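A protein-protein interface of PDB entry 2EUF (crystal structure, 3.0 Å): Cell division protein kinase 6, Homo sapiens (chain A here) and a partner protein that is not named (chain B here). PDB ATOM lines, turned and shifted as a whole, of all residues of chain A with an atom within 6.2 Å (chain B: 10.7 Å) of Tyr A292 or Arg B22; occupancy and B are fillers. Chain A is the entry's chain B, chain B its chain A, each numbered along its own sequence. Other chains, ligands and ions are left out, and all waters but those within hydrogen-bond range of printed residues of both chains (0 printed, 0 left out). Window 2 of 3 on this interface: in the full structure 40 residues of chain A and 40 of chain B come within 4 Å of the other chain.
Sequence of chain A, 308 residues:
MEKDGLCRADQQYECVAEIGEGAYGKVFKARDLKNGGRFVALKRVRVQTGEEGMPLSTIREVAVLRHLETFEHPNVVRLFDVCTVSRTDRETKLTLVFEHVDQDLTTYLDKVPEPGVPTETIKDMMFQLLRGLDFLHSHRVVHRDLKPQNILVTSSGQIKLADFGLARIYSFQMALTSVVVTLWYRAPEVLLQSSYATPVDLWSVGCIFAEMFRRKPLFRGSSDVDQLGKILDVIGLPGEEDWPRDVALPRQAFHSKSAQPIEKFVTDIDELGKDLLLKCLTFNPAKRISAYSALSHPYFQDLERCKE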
ATOM      1  N   LEU A 130     -31.244  -4.760 -14.706  1.00  0.00           N
ATOM      2  CA  LEU A 130     -30.619  -5.527 -13.624  1.00  0.00           C
ATOM      3  C   LEU A 130     -29.095  -5.502 -13.731  1.00  0.00           C
ATOM      4  O   LEU A 130     -28.392  -5.364 -12.722  1.00  0.00           O
ATOM      5  CB  LEU A 130     -31.127  -6.969 -13.600  1.00  0.00           C
ATOM      6  CG  LEU A 130     -32.476  -7.236 -12.930  1.00  0.00           C
ATOM      7  CD1 LEU A 130     -32.971  -8.619 -13.298  1.00  0.00           C
ATOM      8  CD2 LEU A 130     -32.389  -7.089 -11.411  1.00  0.00           C
ATOM      9  N   ASP A 134     -26.529  -4.414 -10.862  1.00  0.00           N
ATOM     10  CA  ASP A 134     -25.487  -5.313 -10.380  1.00  0.00           C
ATOM     11  C   ASP A 134     -24.191  -4.564 -10.198  1.00  0.00           C
ATOM     12  O   ASP A 134     -23.579  -4.586  -9.118  1.00  0.00           O
ATOM     13  CB  ASP A 134     -25.249  -6.415 -11.402  1.00  0.00           C
ATOM     14  CG  ASP A 134     -24.319  -7.505 -10.882  1.00  0.00           C
ATOM     15  OD1 ASP A 134     -24.652  -8.073  -9.813  1.00  0.00           O
ATOM     16  OD2 ASP A 134     -23.262  -7.867 -11.465  1.00  0.00           O
ATOM     17  N   PHE A 135     -23.791  -3.913 -11.287  1.00  0.00           N
ATOM     18  CA  PHE A 135     -22.617  -3.065 -11.343  1.00  0.00           C
ATOM     19  C   PHE A 135     -22.598  -2.125 -10.151  1.00  0.00           C
ATOM     20  O   PHE A 135     -21.743  -2.233  -9.278  1.00  0.00           O
ATOM     21  CB  PHE A 135     -22.625  -2.275 -12.660  1.00  0.00           C
ATOM     22  CG  PHE A 135     -21.469  -1.317 -12.810  1.00  0.00           C
ATOM     23  CD1 PHE A 135     -20.139  -1.793 -12.860  1.00  0.00           C
ATOM     24  CD2 PHE A 135     -21.701   0.060 -12.912  1.00  0.00           C
ATOM     25  CE1 PHE A 135     -19.046  -0.902 -13.005  1.00  0.00           C
ATOM     26  CE2 PHE A 135     -20.627   0.964 -13.051  1.00  0.00           C
ATOM     27  CZ  PHE A 135     -19.292   0.484 -13.097  1.00  0.00           C
ATOM     28  N   SER A 138     -22.206  -3.616  -6.749  1.00  0.00           N
ATOM     29  CA  SER A 138     -20.904  -4.231  -6.499  1.00  0.00           C
ATOM     30  C   SER A 138     -19.823  -3.174  -6.246  1.00  0.00           C
ATOM     31  O   SER A 138     -18.681  -3.511  -5.900  1.00  0.00           O
ATOM     32  CB  SER A 138     -20.505  -5.111  -7.667  1.00  0.00           C
ATOM     33  OG  SER A 138     -20.225  -4.288  -8.772  1.00  0.00           O
ATOM     34  N   SER A 290     -31.190 -10.821  -5.017  1.00  0.00           N
ATOM     35  CA  SER A 290     -30.205  -9.819  -5.429  1.00  0.00           C
ATOM     36  C   SER A 290     -30.111  -9.738  -6.959  1.00  0.00           C
ATOM     37  O   SER A 290     -30.505 -10.682  -7.653  1.00  0.00           O
ATOM     38  CB  SER A 290     -28.839 -10.163  -4.840  1.00  0.00           C
ATOM     39  OG  SER A 290     -28.317 -11.347  -5.423  1.00  0.00           O
ATOM     40  N   ALA A 291     -29.591  -8.622  -7.482  1.00  0.00           N
ATOM     41  CA  ALA A 291     -29.346  -8.479  -8.936  1.00  0.00           C
ATOM     42  C   ALA A 291     -28.547  -9.659  -9.540  1.00  0.00           C
ATOM     43  O   ALA A 291     -28.989 -10.281 -10.505  1.00  0.00           O
ATOM     44  CB  ALA A 291     -28.650  -7.138  -9.247  1.00  0.00           C
ATOM     45  N   TYR A 292     -27.383  -9.950  -8.957  1.00  0.00           N
ATOM     46  CA  TYR A 292     -26.534 -11.057  -9.385  1.00  0.00           C
ATOM     47  C   TYR A 292     -27.276 -12.383  -9.507  1.00  0.00           C
ATOM     48  O   TYR A 292     -27.167 -13.065 -10.539  1.00  0.00           O
ATOM     49  CB  TYR A 292     -25.370 -11.238  -8.420  1.00  0.00           C
ATOM     50  CG  TYR A 292     -24.269 -12.136  -8.944  1.00  0.00           C
ATOM     51  CD1 TYR A 292     -23.490 -11.745 -10.037  1.00  0.00           C
ATOM     52  CD2 TYR A 292     -23.993 -13.358  -8.345  1.00  0.00           C
ATOM     53  CE1 TYR A 292     -22.464 -12.552 -10.532  1.00  0.00           C
ATOM     54  CE2 TYR A 292     -22.961 -14.183  -8.836  1.00  0.00           C
ATOM     55  CZ  TYR A 292     -22.193 -13.771  -9.934  1.00  0.00           C
ATOM     56  OH  TYR A 292     -21.164 -14.566 -10.440  1.00  0.00           O
ATOM     57  N   SER A 293     -28.006 -12.773  -8.462  1.00  0.00           N
ATOM     58  CA  SER A 293     -28.757 -14.021  -8.542  1.00  0.00           C
ATOM     59  C   SER A 293     -29.954 -13.838  -9.456  1.00  0.00           C
ATOM     60  O   SER A 293     -30.326 -14.762 -10.179  1.00  0.00           O
ATOM     61  CB  SER A 293     -29.149 -14.565  -7.170  1.00  0.00           C
ATOM     62  OG  SER A 293     -29.344 -13.530  -6.238  1.00  0.00           O
ATOM     63  N   ALA A 294     -30.528 -12.635  -9.457  1.00  0.00           N
ATOM     64  CA  ALA A 294     -31.612 -12.308 -10.384  1.00  0.00           C
ATOM     65  C   ALA A 294     -31.132 -12.365 -11.827  1.00  0.00           C
ATOM     66  O   ALA A 294     -31.800 -12.943 -12.672  1.00  0.00           O
ATOM     67  CB  ALA A 294     -32.214 -10.948 -10.073  1.00  0.00           C
ATOM     68  N   LEU A 295     -29.966 -11.792 -12.107  1.00  0.00           N
ATOM     69  CA  LEU A 295     -29.389 -11.881 -13.449  1.00  0.00           C
ATOM     70  C   LEU A 295     -29.276 -13.324 -13.940  1.00  0.00           C
ATOM     71  O   LEU A 295     -29.314 -13.571 -15.144  1.00  0.00           O
ATOM     72  CB  LEU A 295     -28.028 -11.176 -13.544  1.00  0.00           C
ATOM     73  CG  LEU A 295     -27.973  -9.662 -13.796  1.00  0.00           C
ATOM     74  CD1 LEU A 295     -26.525  -9.217 -13.957  1.00  0.00           C
ATOM     75  CD2 LEU A 295     -28.787  -9.238 -15.020  1.00  0.00           C
ATOM     76  N   SER A 296     -29.173 -14.266 -13.000  1.00  0.00           N
ATOM     77  CA  SER A 296     -29.044 -15.699 -13.316  1.00  0.00           C
ATOM     78  C   SER A 296     -30.339 -16.508 -13.197  1.00  0.00           C
ATOM     79  O   SER A 296     -30.356 -17.681 -13.541  1.00  0.00           O
ATOM     80  CB  SER A 296     -27.972 -16.341 -12.430  1.00  0.00           C
ATOM     81  OG  SER A 296     -28.442 -16.478 -11.095  1.00  0.00           O
ATOM     82  N   HIS A 297     -31.409 -15.898 -12.696  1.00  0.00           N
ATOM     83  CA  HIS A 297     -32.693 -16.582 -12.601  1.00  0.00           C
ATOM     84  C   HIS A 297     -33.133 -17.070 -13.987  1.00  0.00           C
ATOM     85  O   HIS A 297     -33.065 -16.306 -14.952  1.00  0.00           O
ATOM     86  CB  HIS A 297     -33.756 -15.669 -11.983  1.00  0.00           C
ATOM     87  CG  HIS A 297     -35.103 -16.311 -11.842  1.00  0.00           C
ATOM     88  ND1 HIS A 297     -35.969 -16.473 -12.904  1.00  0.00           N
ATOM     89  CD2 HIS A 297     -35.739 -16.824 -10.760  1.00  0.00           C
ATOM     90  CE1 HIS A 297     -37.073 -17.066 -12.487  1.00  0.00           C
ATOM     91  NE2 HIS A 297     -36.961 -17.287 -11.189  1.00  0.00           N
ATOM     92  N   SER B  15     -25.863  -8.296   2.563  1.00  0.00           N
ATOM     93  CA  SER B  15     -25.005  -9.313   2.025  1.00  0.00           C
ATOM     94  C   SER B  15     -24.505  -8.876   0.661  1.00  0.00           C
ATOM     95  O   SER B  15     -23.351  -9.107   0.328  1.00  0.00           O
ATOM     96  CB  SER B  15     -25.749 -10.614   1.900  1.00  0.00           C
ATOM     97  OG  SER B  15     -26.117 -10.782   0.551  1.00  0.00           O
ATOM     98  N   THR B  16     -25.363  -8.228  -0.117  1.00  0.00           N
ATOM     99  CA  THR B  16     -24.983  -7.816  -1.456  1.00  0.00           C
ATOM    100  C   THR B  16     -23.703  -6.995  -1.433  1.00  0.00           C
ATOM    101  O   THR B  16     -22.766  -7.254  -2.190  1.00  0.00           O
ATOM    102  CB  THR B  16     -26.093  -6.987  -2.099  1.00  0.00           C
ATOM    103  OG1 THR B  16     -27.187  -7.838  -2.482  1.00  0.00           O
ATOM    104  CG2 THR B  16     -25.610  -6.418  -3.422  1.00  0.00           C
ATOM    105  N   THR B  17     -23.681  -6.011  -0.544  1.00  0.00           N
ATOM    106  CA  THR B  17     -22.640  -4.992  -0.467  1.00  0.00           C
ATOM    107  C   THR B  17     -21.489  -5.460   0.398  1.00  0.00           C
ATOM    108  O   THR B  17     -20.387  -4.920   0.323  1.00  0.00           O
ATOM    109  CB  THR B  17     -23.291  -3.646   0.051  1.00  0.00           C
ATOM    110  OG1 THR B  17     -23.440  -2.736  -1.050  1.00  0.00           O
ATOM    111  CG2 THR B  17     -22.424  -2.851   1.079  1.00  0.00           C
ATOM    112  N   MET B  18     -21.730  -6.479   1.213  1.00  0.00           N
ATOM    113  CA  MET B  18     -20.734  -6.866   2.209  1.00  0.00           C
ATOM    114  C   MET B  18     -20.114  -8.271   2.060  1.00  0.00           C
ATOM    115  O   MET B  18     -18.960  -8.474   2.396  1.00  0.00           O
ATOM    116  CB  MET B  18     -21.285  -6.628   3.620  1.00  0.00           C
ATOM    117  CG  MET B  18     -21.405  -5.152   3.982  1.00  0.00           C
ATOM    118  SD  MET B  18     -22.704  -4.840   5.193  1.00  0.00           S
ATOM    119  CE  MET B  18     -22.931  -3.071   5.020  1.00  0.00           C
ATOM    120  N   LYS B  19     -20.851  -9.240   1.552  1.00  0.00           N
ATOM    121  CA  LYS B  19     -20.316 -10.582   1.529  1.00  0.00           C
ATOM    122  C   LYS B  19     -19.943 -11.017   0.123  1.00  0.00           C
ATOM    123  O   LYS B  19     -19.344 -12.090  -0.054  1.00  0.00           O
ATOM    124  CB  LYS B  19     -21.318 -11.577   2.119  1.00  0.00           C
ATOM    125  CG  LYS B  19     -21.505 -11.521   3.625  1.00  0.00           C
ATOM    126  CD  LYS B  19     -22.692 -12.424   3.998  1.00  0.00           C
ATOM    127  CE  LYS B  19     -22.671 -12.833   5.459  1.00  0.00           C
ATOM    128  NZ  LYS B  19     -21.392 -13.574   5.821  1.00  0.00           N
ATOM    129  N   ASP B  20     -20.322 -10.214  -0.873  1.00  0.00           N
ATOM    130  CA  ASP B  20     -19.964 -10.492  -2.271  1.00  0.00           C
ATOM    131  C   ASP B  20     -18.437 -10.343  -2.446  1.00  0.00           C
ATOM    132  O   ASP B  20     -17.884  -9.256  -2.233  1.00  0.00           O
ATOM    133  CB  ASP B  20     -20.745  -9.575  -3.230  1.00  0.00           C
ATOM    134  CG  ASP B  20     -20.464  -9.868  -4.717  1.00  0.00           C
ATOM    135  OD1 ASP B  20     -19.485 -10.586  -5.031  1.00  0.00           O
ATOM    136  OD2 ASP B  20     -21.175  -9.404  -5.649  1.00  0.00           O
ATOM    137  N   PRO B  21     -17.754 -11.433  -2.803  1.00  0.00           N
ATOM    138  CA  PRO B  21     -16.316 -11.391  -2.947  1.00  0.00           C
ATOM    139  C   PRO B  21     -15.922 -10.318  -3.941  1.00  0.00           C
ATOM    140  O   PRO B  21     -14.883  -9.653  -3.744  1.00  0.00           O
ATOM    141  CB  PRO B  21     -15.969 -12.775  -3.478  1.00  0.00           C
ATOM    142  CG  PRO B  21     -17.212 -13.300  -3.994  1.00  0.00           C
ATOM    143  CD  PRO B  21     -18.285 -12.774  -3.101  1.00  0.00           C
ATOM    144  N   ARG B  22     -16.748 -10.110  -4.971  1.00  0.00           N
ATOM    145  CA  ARG B  22     -16.352  -9.157  -6.004  1.00  0.00           C
ATOM    146  C   ARG B  22     -16.438  -7.709  -5.554  1.00  0.00           C
ATOM    147  O   ARG B  22     -15.770  -6.815  -6.093  1.00  0.00           O
ATOM    148  CB  ARG B  22     -16.971  -9.432  -7.375  1.00  0.00           C
ATOM    149  CG  ARG B  22     -18.373  -9.206  -7.508  1.00  0.00           C
ATOM    150  CD  ARG B  22     -18.988 -10.161  -8.433  1.00  0.00           C
ATOM    151  NE  ARG B  22     -20.431 -10.048  -8.284  1.00  0.00           N
ATOM    152  CZ  ARG B  22     -21.194  -9.226  -8.987  1.00  0.00           C
ATOM    153  NH1 ARG B  22     -20.671  -8.437  -9.916  1.00  0.00           N
ATOM    154  NH2 ARG B  22     -22.486  -9.195  -8.763  1.00  0.00           N
ATOM    155  N   VAL B  23     -17.198  -7.487  -4.501  1.00  0.00           N
ATOM    156  CA  VAL B  23     -17.078  -6.206  -3.836  1.00  0.00           C
ATOM    157  C   VAL B  23     -15.615  -5.978  -3.421  1.00  0.00           C
ATOM    158  O   VAL B  23     -15.047  -4.948  -3.793  1.00  0.00           O
ATOM    159  CB  VAL B  23     -18.097  -6.033  -2.695  1.00  0.00           C
ATOM    160  CG1 VAL B  23     -17.899  -4.708  -2.012  1.00  0.00           C
ATOM    161  CG2 VAL B  23     -19.502  -6.121  -3.275  1.00  0.00           C
ATOM    162  N   LEU B  24     -15.008  -6.940  -2.716  1.00  0.00           N
ATOM    163  CA  LEU B  24     -13.641  -6.763  -2.204  1.00  0.00           C
ATOM    164  C   LEU B  24     -12.728  -6.519  -3.375  1.00  0.00           C
ATOM    165  O   LEU B  24     -11.787  -5.718  -3.348  1.00  0.00           O
ATOM    166  CB  LEU B  24     -13.144  -8.021  -1.492  1.00  0.00           C
ATOM    167  CG  LEU B  24     -12.192  -7.859  -0.295  1.00  0.00           C
ATOM    168  CD1 LEU B  24     -11.459  -9.154  -0.018  1.00  0.00           C
ATOM    169  CD2 LEU B  24     -11.222  -6.719  -0.463  1.00  0.00           C
ATOM    170  N   ASN B  25     -13.052  -7.254  -4.416  1.00  0.00           N
ATOM    171  CA  ASN B  25     -12.330  -7.274  -5.653  1.00  0.00           C
ATOM    172  C   ASN B  25     -12.298  -5.876  -6.291  1.00  0.00           C
ATOM    173  O   ASN B  25     -11.264  -5.456  -6.792  1.00  0.00           O
ATOM    174  CB  ASN B  25     -13.070  -8.280  -6.519  1.00  0.00           C
ATOM    175  CG  ASN B  25     -12.273  -8.782  -7.666  1.00  0.00           C
ATOM    176  OD1 ASN B  25     -11.071  -8.476  -7.819  1.00  0.00           O
ATOM    177  ND2 ASN B  25     -12.950  -9.584  -8.519  1.00  0.00           N
ATOM    178  N   ASN B  26     -13.420  -5.151  -6.238  1.00  0.00           N
ATOM    179  CA  ASN B  26     -13.512  -3.828  -6.867  1.00  0.00           C
ATOM    180  C   ASN B  26     -12.920  -2.723  -6.032  1.00  0.00           C
ATOM    181  O   ASN B  26     -12.498  -1.719  -6.577  1.00  0.00           O
ATOM    182  CB  ASN B  26     -14.951  -3.448  -7.194  1.00  0.00           C
ATOM    183  CG  ASN B  26     -15.639  -4.447  -8.073  1.00  0.00           C
ATOM    184  OD1 ASN B  26     -15.059  -4.981  -9.020  1.00  0.00           O
ATOM    185  ND2 ASN B  26     -16.902  -4.698  -7.777  1.00  0.00           N
ATOM    186  N   LEU B  27     -12.924  -2.881  -4.713  1.00  0.00           N
ATOM    187  CA  LEU B  27     -12.267  -1.898  -3.850  1.00  0.00           C
ATOM    188  C   LEU B  27     -10.778  -1.810  -4.195  1.00  0.00           C
ATOM    189  O   LEU B  27     -10.232  -0.716  -4.406  1.00  0.00           O
ATOM    190  CB  LEU B  27     -12.468  -2.214  -2.363  1.00  0.00           C
ATOM    191  CG  LEU B  27     -13.687  -1.533  -1.736  1.00  0.00           C
ATOM    192  CD1 LEU B  27     -13.895  -1.927  -0.286  1.00  0.00           C
ATOM    193  CD2 LEU B  27     -13.603  -0.031  -1.858  1.00  0.00           C
ATOM    194  N   LYS B  28     -10.159  -2.987  -4.279  1.00  0.00           N
ATOM    195  CA  LYS B  28      -8.784  -3.151  -4.660  1.00  0.00           C
ATOM    196  C   LYS B  28      -8.547  -2.541  -6.028  1.00  0.00           C
ATOM    197  O   LYS B  28      -7.538  -1.856  -6.234  1.00  0.00           O
ATOM    198  CB  LYS B  28      -8.431  -4.634  -4.648  1.00  0.00           C
ATOM    199  CG  LYS B  28      -8.410  -5.234  -3.242  1.00  0.00           C
ATOM    200  CD  LYS B  28      -8.541  -6.753  -3.244  1.00  0.00           C
ATOM    201  CE  LYS B  28      -7.224  -7.451  -3.542  1.00  0.00           C
ATOM    202  NZ  LYS B  28      -7.429  -8.903  -3.798  1.00  0.00           N
ATOM    203  N   LEU B  29      -9.479  -2.763  -6.951  1.00  0.00           N
ATOM    204  CA  LEU B  29      -9.383  -2.187  -8.288  1.00  0.00           C
ATOM    205  C   LEU B  29      -9.465  -0.669  -8.256  1.00  0.00           C
ATOM    206  O   LEU B  29      -8.602   0.008  -8.787  1.00  0.00           O
ATOM    207  CB  LEU B  29     -10.473  -2.761  -9.195  1.00  0.00           C
ATOM    208  CG  LEU B  29     -10.029  -3.902 -10.108  1.00  0.00           C
ATOM    209  CD1 LEU B  29     -10.910  -5.143 -10.001  1.00  0.00           C
ATOM    210  CD2 LEU B  29      -9.978  -3.408 -11.528  1.00  0.00           C
ATOM    211  N   ARG B  30     -10.495  -0.133  -7.610  1.00  0.00           N
ATOM    212  CA  ARG B  30     -10.730   1.311  -7.634  1.00  0.00           C
ATOM    213  C   ARG B  30      -9.710   2.055  -6.776  1.00  0.00           C
ATOM    214  O   ARG B  30      -9.544   3.269  -6.907  1.00  0.00           O
ATOM    215  CB  ARG B  30     -12.155   1.650  -7.206  1.00  0.00           C
ATOM    216  CG  ARG B  30     -13.239   1.160  -8.164  1.00  0.00           C
ATOM    217  CD  ARG B  30     -14.639   1.720  -7.884  1.00  0.00           C
ATOM    218  NE  ARG B  30     -14.878   1.991  -6.460  1.00  0.00           N
ATOM    219  CZ  ARG B  30     -15.292   1.096  -5.562  1.00  0.00           C
ATOM    220  NH1 ARG B  30     -15.530  -0.160  -5.913  1.00  0.00           N
ATOM    221  NH2 ARG B  30     -15.468   1.461  -4.299  1.00  0.00           N
ATOM    222  N   GLU B  31      -9.047   1.308  -5.890  1.00  0.00           N
ATOM    223  CA  GLU B  31      -7.833   1.735  -5.190  1.00  0.00           C
ATOM    224  C   GLU B  31      -6.751   2.064  -6.211  1.00  0.00           C
ATOM    225  O   GLU B  31      -6.032   3.033  -6.044  1.00  0.00           O
ATOM    226  CB  GLU B  31      -7.368   0.607  -4.285  1.00  0.00           C
ATOM    227  CG  GLU B  31      -6.285   0.926  -3.278  1.00  0.00           C
ATOM    228  CD  GLU B  31      -6.172  -0.160  -2.196  1.00  0.00           C
ATOM    229  OE1 GLU B  31      -5.476   0.055  -1.175  1.00  0.00           O
ATOM    230  OE2 GLU B  31      -6.780  -1.248  -2.355  1.00  0.00           O
ATOM    231  N   ASP B 154     -13.545   1.849   3.858  1.00  0.00           N
ATOM    232  CA  ASP B 154     -14.455   1.081   3.016  1.00  0.00           C
ATOM    233  C   ASP B 154     -14.161  -0.422   3.097  1.00  0.00           C
ATOM    234  O   ASP B 154     -15.050  -1.239   2.863  1.00  0.00           O
ATOM    235  CB  ASP B 154     -14.416   1.584   1.567  1.00  0.00           C
ATOM    236  CG  ASP B 154     -14.966   3.016   1.402  1.00  0.00           C
ATOM    237  OD1 ASP B 154     -15.926   3.414   2.117  1.00  0.00           O
ATOM    238  OD2 ASP B 154     -14.498   3.809   0.547  1.00  0.00           O
ATOM    239  N   PHE B 155     -12.921  -0.765   3.467  1.00  0.00           N
ATOM    240  CA  PHE B 155     -12.445  -2.145   3.485  1.00  0.00           C
ATOM    241  C   PHE B 155     -12.813  -2.925   4.732  1.00  0.00           C
ATOM    242  O   PHE B 155     -12.619  -4.140   4.764  1.00  0.00           O
ATOM    243  CB  PHE B 155     -10.929  -2.186   3.373  1.00  0.00           C
ATOM    244  CG  PHE B 155     -10.401  -2.070   1.962  1.00  0.00           C
ATOM    245  CD1 PHE B 155     -10.172  -0.820   1.385  1.00  0.00           C
ATOM    246  CD2 PHE B 155     -10.084  -3.221   1.229  1.00  0.00           C
ATOM    247  CE1 PHE B 155      -9.674  -0.715   0.112  1.00  0.00           C
ATOM    248  CE2 PHE B 155      -9.578  -3.119  -0.059  1.00  0.00           C
ATOM    249  CZ  PHE B 155      -9.375  -1.858  -0.614  1.00  0.00           C
ATOM    250  N   PRO B 158     -15.760  -5.844   4.318  1.00  0.00           N
ATOM    251  CA  PRO B 158     -15.210  -6.737   3.311  1.00  0.00           C
ATOM    252  C   PRO B 158     -13.986  -7.514   3.805  1.00  0.00           C
ATOM    253  O   PRO B 158     -13.806  -8.655   3.395  1.00  0.00           O
ATOM    254  CB  PRO B 158     -14.844  -5.792   2.164  1.00  0.00           C
ATOM    255  CG  PRO B 158     -15.837  -4.697   2.272  1.00  0.00           C
ATOM    256  CD  PRO B 158     -16.020  -4.509   3.749  1.00  0.00           C
ATOM    257  N   ASN B 161     -15.435 -10.078   6.565  1.00  0.00           N
ATOM    258  CA  ASN B 161     -16.039 -11.139   5.795  1.00  0.00           C
ATOM    259  C   ASN B 161     -15.032 -12.073   5.158  1.00  0.00           C
ATOM    260  O   ASN B 161     -15.147 -13.282   5.276  1.00  0.00           O
ATOM    261  CB  ASN B 161     -16.905 -10.563   4.696  1.00  0.00           C
ATOM    262  CG  ASN B 161     -17.650 -11.638   3.936  1.00  0.00           C
ATOM    263  OD1 ASN B 161     -18.554 -12.286   4.472  1.00  0.00           O
ATOM    264  ND2 ASN B 161     -17.274 -11.834   2.686  1.00  0.00           N
ATOM    265  N   ALA B 162     -14.054 -11.507   4.468  1.00  0.00           N
ATOM    266  CA  ALA B 162     -13.061 -12.313   3.794  1.00  0.00           C
ATOM    267  C   ALA B 162     -12.281 -13.181   4.786  1.00  0.00           C
ATOM    268  O   ALA B 162     -11.930 -14.322   4.476  1.00  0.00           O
ATOM    269  CB  ALA B 162     -12.132 -11.439   3.006  1.00  0.00           C
ATOM    270  N   ILE B 227      -5.411 -12.175   0.997  1.00  0.00           N
ATOM    271  CA  ILE B 227      -6.524 -11.322   0.567  1.00  0.00           C
ATOM    272  C   ILE B 227      -6.029 -10.134  -0.268  1.00  0.00           C
ATOM    273  O   ILE B 227      -6.429  -9.999  -1.428  1.00  0.00           O
ATOM    274  CB  ILE B 227      -7.361 -10.783   1.775  1.00  0.00           C
ATOM    275  CG1 ILE B 227      -7.751 -11.887   2.774  1.00  0.00           C
ATOM    276  CG2 ILE B 227      -8.562 -10.008   1.290  1.00  0.00           C
ATOM    277  CD1 ILE B 227      -8.503 -13.040   2.192  1.00  0.00           C
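The side-chain amide nitrogen of Asn B26 lies within hydrogen-bond range of the backbone carbonyl oxygen of Ser A138 (2.8 Å). The guanidinium group (NH2) of Arg B22 is in salt-bridge range of the side-chain carboxylate (OD1) of Asp A134 (2.7 Å).
The side-chain amide nitrogen (ND2) of Asn B26 is in hydrogen-bond range of the backbone carbonyl oxygen (O) of Arg B22 (2.9 Å). The side-chain hydroxyl (OG) of Ser A290 lies within hydrogen-bond range of the side-chain hydroxyl (OG) of Ser A293, 2.5 Å away. The side-chain carboxylate (OD2) of Asp B20 lies within salt-bridge range of the guanidinium group (NE) of Arg B22 (2.8 Å). The side-chain carboxylate (OD1) of Asp A134 lies within hydrogen-bond range of the backbone NH (N) of Tyr A292 (3.4 Å). The backbone carbonyl oxygen (O) of Phe A135 lies within hydrogen-bond range of the side-chain hydroxyl (OG) of Ser A138 (2.6 Å). The backbone carbonyl oxygen (O) of Asn B26 lies close to the guanidinium group (NH1) of Arg B30 (3.5 Å).
Among the printed residues, pairs that only touch across the chains: Ser A138 with Val B23 (3.8 Å), Ser A290 with Thr B16 (3.7 Å) and Tyr A292 with Arg B22 (3.0 Å).
Asp A134 touches just one residue of chain B: Arg B22 (2.7 Å). Of the printed residues of chain B, Ser A290 touches Thr B16. No residue of chain B comes within 4 Å of Ala A291. No residue of chain B comes within 4 Å of Ala A294. No residue of chain B comes within 4 Å of Leu A295. Printed residues of chain A within 4 Å of Thr B16: Ser A290 (3.7 Å). Of the printed residues of chain A, Arg B22 touches Asp A134 (2.7 Å) and Tyr A292 (3.0 Å). Printed residues of chain A within 4 Å of Val B23: Ser A138. The nearest printed residue of chain A that does not touch Arg B22 is Ser A138 (4.02 Å). The nearest printed residue of chain A that does not touch Val B23 is Asp A134 (7.3 Å).
Of the 23 printed residues of chain B, 4 touch a printed residue of chain A. Hydrophobic or aromatic side chains of chain B within 4 Å of the printed part of chain A: Val B23. Of the 12 printed residues of chain A, 4 touch a printed residue of chain B.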
